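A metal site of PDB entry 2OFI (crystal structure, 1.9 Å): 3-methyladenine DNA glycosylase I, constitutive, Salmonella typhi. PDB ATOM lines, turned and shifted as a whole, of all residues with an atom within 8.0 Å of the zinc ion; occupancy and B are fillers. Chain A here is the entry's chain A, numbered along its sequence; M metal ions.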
ATOM      1  N   GLN A   2       5.625  -1.035  16.229  1.00  0.00           N
ATOM      2  CA  GLN A   2       6.382   0.209  16.405  1.00  0.00           C
ATOM      3  C   GLN A   2       7.882  -0.082  16.264  1.00  0.00           C
ATOM      4  O   GLN A   2       8.369  -1.020  16.866  1.00  0.00           O
ATOM      5  CB  GLN A   2       6.086   0.871  17.757  1.00  0.00           C
ATOM      6  N   ARG A   3       8.582   0.712  15.457  1.00  0.00           N
ATOM      7  CA  ARG A   3      10.008   0.495  15.215  1.00  0.00           C
ATOM      8  C   ARG A   3      10.784   1.783  15.462  1.00  0.00           C
ATOM      9  O   ARG A   3      10.192   2.827  15.722  1.00  0.00           O
ATOM     10  CB  ARG A   3      10.247   0.019  13.776  1.00  0.00           C
ATOM     11  CG  ARG A   3       9.724  -1.380  13.478  1.00  0.00           C
ATOM     12  CD  ARG A   3      10.011  -1.737  12.005  1.00  0.00           C
ATOM     13  NE  ARG A   3       9.650  -3.132  11.741  1.00  0.00           N
ATOM     14  CZ  ARG A   3       8.451  -3.557  11.366  1.00  0.00           C
ATOM     15  NH1 ARG A   3       7.429  -2.720  11.227  1.00  0.00           N
ATOM     16  NH2 ARG A   3       8.263  -4.848  11.159  1.00  0.00           N
ATOM     17  N   CYS A   4      12.108   1.712  15.411  1.00  0.00           N
ATOM     18  CA  CYS A   4      12.957   2.891  15.590  1.00  0.00           C
ATOM     19  C   CYS A   4      12.612   3.946  14.534  1.00  0.00           C
ATOM     20  O   CYS A   4      12.099   3.622  13.445  1.00  0.00           O
ATOM     21  CB  CYS A   4      14.416   2.478  15.460  1.00  0.00           C
ATOM     22  SG  CYS A   4      15.015   1.512  16.835  1.00  0.00           S
ATOM     23  N   ASP A   5      12.942   5.200  14.844  1.00  0.00           N
ATOM     24  CA  ASP A   5      12.556   6.357  14.048  1.00  0.00           C
ATOM     25  C   ASP A   5      13.148   6.358  12.651  1.00  0.00           C
ATOM     26  O   ASP A   5      12.527   6.893  11.735  1.00  0.00           O
ATOM     27  CB  ASP A   5      12.993   7.640  14.774  1.00  0.00           C
ATOM     28  CG  ASP A   5      12.387   7.732  16.167  1.00  0.00           C
ATOM     29  OD1 ASP A   5      11.169   7.461  16.283  1.00  0.00           O
ATOM     30  OD2 ASP A   5      13.120   8.003  17.143  1.00  0.00           O
ATOM     31  N   TRP A   6      14.341   5.807  12.490  1.00  0.00           N
ATOM     32  CA  TRP A   6      15.064   5.905  11.233  1.00  0.00           C
ATOM     33  C   TRP A   6      14.616   4.872  10.202  1.00  0.00           C
ATOM     34  O   TRP A   6      15.052   4.895   9.053  1.00  0.00           O
ATOM     35  CB  TRP A   6      16.562   5.814  11.495  1.00  0.00           C
ATOM     36  CG  TRP A   6      16.956   4.671  12.431  1.00  0.00           C
ATOM     37  CD1 TRP A   6      17.169   4.769  13.794  1.00  0.00           C
ATOM     38  CD2 TRP A   6      17.176   3.303  12.098  1.00  0.00           C
ATOM     39  NE1 TRP A   6      17.506   3.537  14.318  1.00  0.00           N
ATOM     40  CE2 TRP A   6      17.489   2.611  13.298  1.00  0.00           C
ATOM     41  CE3 TRP A   6      17.103   2.559  10.895  1.00  0.00           C
ATOM     42  CZ2 TRP A   6      17.796   1.257  13.320  1.00  0.00           C
ATOM     43  CZ3 TRP A   6      17.395   1.187  10.937  1.00  0.00           C
ATOM     44  CH2 TRP A   6      17.711   0.557  12.141  1.00  0.00           C
ATOM     45  N   VAL A   7      13.713   3.973  10.576  1.00  0.00           N
ATOM     46  CA  VAL A   7      13.371   2.885   9.663  1.00  0.00           C
ATOM     47  C   VAL A   7      12.358   3.465   8.689  1.00  0.00           C
ATOM     48  O   VAL A   7      11.350   4.000   9.117  1.00  0.00           O
ATOM     49  CB  VAL A   7      12.749   1.652  10.390  1.00  0.00           C
ATOM     50  CG1 VAL A   7      12.526   0.473   9.391  1.00  0.00           C
ATOM     51  CG2 VAL A   7      13.683   1.163  11.535  1.00  0.00           C
ATOM     52  N   HIS A  17      16.512  -3.810   9.949  1.00  0.00           N
ATOM     53  CA  HIS A  17      16.253  -3.369  11.320  1.00  0.00           C
ATOM     54  C   HIS A  17      15.810  -4.501  12.219  1.00  0.00           C
ATOM     55  O   HIS A  17      16.230  -4.623  13.388  1.00  0.00           O
ATOM     56  CB  HIS A  17      15.130  -2.314  11.337  1.00  0.00           C
ATOM     57  CG  HIS A  17      14.567  -2.065  12.705  1.00  0.00           C
ATOM     58  ND1 HIS A  17      13.508  -2.772  13.201  1.00  0.00           N
ATOM     59  CD2 HIS A  17      14.945  -1.200  13.680  1.00  0.00           C
ATOM     60  CE1 HIS A  17      13.228  -2.344  14.425  1.00  0.00           C
ATOM     61  NE2 HIS A  17      14.104  -1.411  14.747  1.00  0.00           N
ATOM     62  N   ASP A  18      14.869  -5.300  11.736  1.00  0.00           N
ATOM     63  CA  ASP A  18      14.251  -6.307  12.584  1.00  0.00           C
ATOM     64  C   ASP A  18      15.177  -7.483  12.864  1.00  0.00           C
ATOM     65  O   ASP A  18      15.109  -8.106  13.924  1.00  0.00           O
ATOM     66  CB  ASP A  18      13.009  -6.909  11.899  1.00  0.00           C
ATOM     67  CG  ASP A  18      11.815  -5.946  11.814  1.00  0.00           C
ATOM     68  OD1 ASP A  18      11.900  -4.764  12.233  1.00  0.00           O
ATOM     69  OD2 ASP A  18      10.762  -6.379  11.251  1.00  0.00           O
ATOM     70  N   TRP A  21      20.090  -5.299  12.807  1.00  0.00           N
ATOM     71  CA  TRP A  21      20.631  -4.152  13.493  1.00  0.00           C
ATOM     72  C   TRP A  21      20.544  -4.303  15.019  1.00  0.00           C
ATOM     73  O   TRP A  21      19.460  -4.609  15.528  1.00  0.00           O
ATOM     74  CB  TRP A  21      19.880  -2.901  13.070  1.00  0.00           C
ATOM     75  CG  TRP A  21      20.534  -1.595  13.480  1.00  0.00           C
ATOM     76  CD1 TRP A  21      21.532  -0.921  12.822  1.00  0.00           C
ATOM     77  CD2 TRP A  21      20.142  -0.790  14.585  1.00  0.00           C
ATOM     78  NE1 TRP A  21      21.816   0.252  13.485  1.00  0.00           N
ATOM     79  CE2 TRP A  21      20.973   0.367  14.572  1.00  0.00           C
ATOM     80  CE3 TRP A  21      19.187  -0.946  15.642  1.00  0.00           C
ATOM     81  CZ2 TRP A  21      20.844   1.405  15.519  1.00  0.00           C
ATOM     82  CZ3 TRP A  21      19.043   0.104  16.576  1.00  0.00           C
ATOM     83  CH2 TRP A  21      19.889   1.271  16.497  1.00  0.00           C
ATOM     84  N   ASN A 173      23.071  -1.394  22.230  1.00  0.00           N
ATOM     85  CA  ASN A 173      21.748  -1.722  21.731  1.00  0.00           C
ATOM     86  C   ASN A 173      20.940  -0.449  21.775  1.00  0.00           C
ATOM     87  O   ASN A 173      20.504  -0.024  22.848  1.00  0.00           O
ATOM     88  CB  ASN A 173      21.129  -2.821  22.609  1.00  0.00           C
ATOM     89  CG  ASN A 173      19.797  -3.340  22.085  1.00  0.00           C
ATOM     90  OD1 ASN A 173      19.409  -4.513  22.364  1.00  0.00           O
ATOM     91  ND2 ASN A 173      19.054  -2.491  21.388  1.00  0.00           N
ATOM     92  N   ASP A 174      20.788   0.193  20.617  1.00  0.00           N
ATOM     93  CA  ASP A 174      20.159   1.518  20.565  1.00  0.00           C
ATOM     94  C   ASP A 174      18.743   1.496  19.945  1.00  0.00           C
ATOM     95  O   ASP A 174      18.296   2.489  19.421  1.00  0.00           O
ATOM     96  CB  ASP A 174      21.056   2.531  19.817  1.00  0.00           C
ATOM     97  CG  ASP A 174      22.119   3.212  20.728  1.00  0.00           C
ATOM     98  OD1 ASP A 174      22.047   3.082  21.958  1.00  0.00           O
ATOM     99  OD2 ASP A 174      23.050   3.887  20.193  1.00  0.00           O
ATOM    100  N   HIS A 175      18.042   0.377  20.010  1.00  0.00           N
ATOM    101  CA  HIS A 175      16.642   0.331  19.635  1.00  0.00           C
ATOM    102  C   HIS A 175      15.913   1.202  20.663  1.00  0.00           C
ATOM    103  O   HIS A 175      16.062   0.971  21.842  1.00  0.00           O
ATOM    104  CB  HIS A 175      16.103  -1.087  19.815  1.00  0.00           C
ATOM    105  CG  HIS A 175      16.461  -1.982  18.686  1.00  0.00           C
ATOM    106  ND1 HIS A 175      15.879  -1.853  17.443  1.00  0.00           N
ATOM    107  CD2 HIS A 175      17.372  -2.982  18.589  1.00  0.00           C
ATOM    108  CE1 HIS A 175      16.369  -2.806  16.637  1.00  0.00           C
ATOM    109  NE2 HIS A 175      17.279  -3.489  17.313  1.00  0.00           N
ATOM    110  N   ILE A 176      15.170   2.203  20.206  1.00  0.00           N
ATOM    111  CA  ILE A 176      14.485   3.086  21.204  1.00  0.00           C
ATOM    112  C   ILE A 176      13.512   2.308  22.096  1.00  0.00           C
ATOM    113  O   ILE A 176      13.016   1.236  21.715  1.00  0.00           O
ATOM    114  CB  ILE A 176      13.722   4.240  20.525  1.00  0.00           C
ATOM    115  CG1 ILE A 176      12.777   3.682  19.434  1.00  0.00           C
ATOM    116  CG2 ILE A 176      14.702   5.259  19.970  1.00  0.00           C
ATOM    117  CD1 ILE A 176      11.781   4.758  18.817  1.00  0.00           C
ATOM    118  N   THR A 177      13.214   2.862  23.272  1.00  0.00           N
ATOM    119  CA  THR A 177      12.392   2.130  24.264  1.00  0.00           C
ATOM    120  C   THR A 177      11.032   1.625  23.719  1.00  0.00           C
ATOM    121  O   THR A 177      10.557   0.560  24.144  1.00  0.00           O
ATOM    122  CB  THR A 177      12.163   2.941  25.552  1.00  0.00           C
ATOM    123  OG1 THR A 177      11.613   4.207  25.209  1.00  0.00           O
ATOM    124  CG2 THR A 177      13.502   3.184  26.248  1.00  0.00           C
ATOM    125  N   GLY A 178      10.428   2.399  22.807  1.00  0.00           N
ATOM    126  CA  GLY A 178       9.126   2.030  22.239  1.00  0.00           C
ATOM    127  C   GLY A 178       9.198   1.087  21.043  1.00  0.00           C
ATOM    128  O   GLY A 178       8.158   0.612  20.562  1.00  0.00           O
ATOM    129  N   CYS A 179      10.409   0.791  20.570  1.00  0.00           N
ATOM    130  CA  CYS A 179      10.594  -0.166  19.459  1.00  0.00           C
ATOM    131  C   CYS A 179      10.302  -1.604  19.900  1.00  0.00           C
ATOM    132  O   CYS A 179      10.710  -2.049  20.990  1.00  0.00           O
ATOM    133  CB  CYS A 179      12.017  -0.076  18.934  1.00  0.00           C
ATOM    134  SG  CYS A 179      12.325  -1.254  17.532  1.00  0.00           S
ATOM    135  N   PHE A 180       9.589  -2.362  19.071  1.00  0.00           N
ATOM    136  CA  PHE A 180       9.290  -3.748  19.473  1.00  0.00           C
ATOM    137  C   PHE A 180      10.557  -4.623  19.711  1.00  0.00           C
ATOM    138  O   PHE A 180      10.468  -5.672  20.348  1.00  0.00           O
ATOM    139  CB  PHE A 180       8.331  -4.417  18.475  1.00  0.00           C
ATOM    140  CG  PHE A 180       9.000  -5.051  17.289  1.00  0.00           C
ATOM    141  CD1 PHE A 180       9.245  -6.434  17.245  1.00  0.00           C
ATOM    142  CD2 PHE A 180       9.325  -4.295  16.165  1.00  0.00           C
ATOM    143  CE1 PHE A 180       9.863  -7.048  16.120  1.00  0.00           C
ATOM    144  CE2 PHE A 180       9.920  -4.890  15.041  1.00  0.00           C
ATOM    145  CZ  PHE A 180      10.190  -6.268  15.023  1.00  0.00           C
ATOM    146  N   CYS A 181      11.697  -4.214  19.150  1.00  0.00           N
ATOM    147  CA  CYS A 181      12.960  -4.938  19.331  1.00  0.00           C
ATOM    148  C   CYS A 181      13.722  -4.513  20.584  1.00  0.00           C
ATOM    149  O   CYS A 181      14.731  -5.150  20.938  1.00  0.00           O
ATOM    150  CB  CYS A 181      13.882  -4.767  18.137  1.00  0.00           C
ATOM    151  SG  CYS A 181      13.290  -5.430  16.556  1.00  0.00           S
ATOM    152  N   HIS A 182      13.280  -3.446  21.258  1.00  0.00           N
ATOM    153  CA  HIS A 182      13.910  -3.052  22.505  1.00  0.00           C
ATOM    154  C   HIS A 182      13.832  -4.156  23.530  1.00  0.00           C
ATOM    155  O   HIS A 182      12.748  -4.720  23.729  1.00  0.00           O
ATOM    156  CB  HIS A 182      13.246  -1.840  23.113  1.00  0.00           C
ATOM    157  CG  HIS A 182      14.064  -1.206  24.193  1.00  0.00           C
ATOM    158  ND1 HIS A 182      13.835  -1.451  25.530  1.00  0.00           N
ATOM    159  CD2 HIS A 182      15.104  -0.342  24.136  1.00  0.00           C
ATOM    160  CE1 HIS A 182      14.675  -0.737  26.251  1.00  0.00           C
ATOM    161  NE2 HIS A 182      15.485  -0.077  25.435  1.00  0.00           N
HETATM  162 ZN    ZN M   1      14.348  -0.659  16.685  1.00  0.00          ZN
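The backbone NH of Cys 181 lies close to the side-chain sulfur of Cys 179 (3.4 Å).
OD1 of Asp 18 is in hydrogen-bond range of ND1 of His 17 (2.7 Å).
A ring nitrogen (NE2) of His 175 lies within hydrogen-bond range of the backbone carbonyl oxygen (O) of Trp 21 (3.0 Å).
The backbone NH (N) of Ile 176 sits close to the side-chain sulfur (SG) of Cys 4 (3.4 Å).
N of His 175 sits close to ND2 of Asn 173 (3.3 Å).
ND1 of His 175 is bound to the zinc ion (2.1 Å).
NE2 of His 17 is bound to the zinc ion (2.1 Å).
SG of Cys 179 is bound to the zinc ion, at 2.3 Å.
SG of Cys 4 is bound to the zinc ion (2.3 Å).
The zinc ion has four donor atoms within binding distance.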
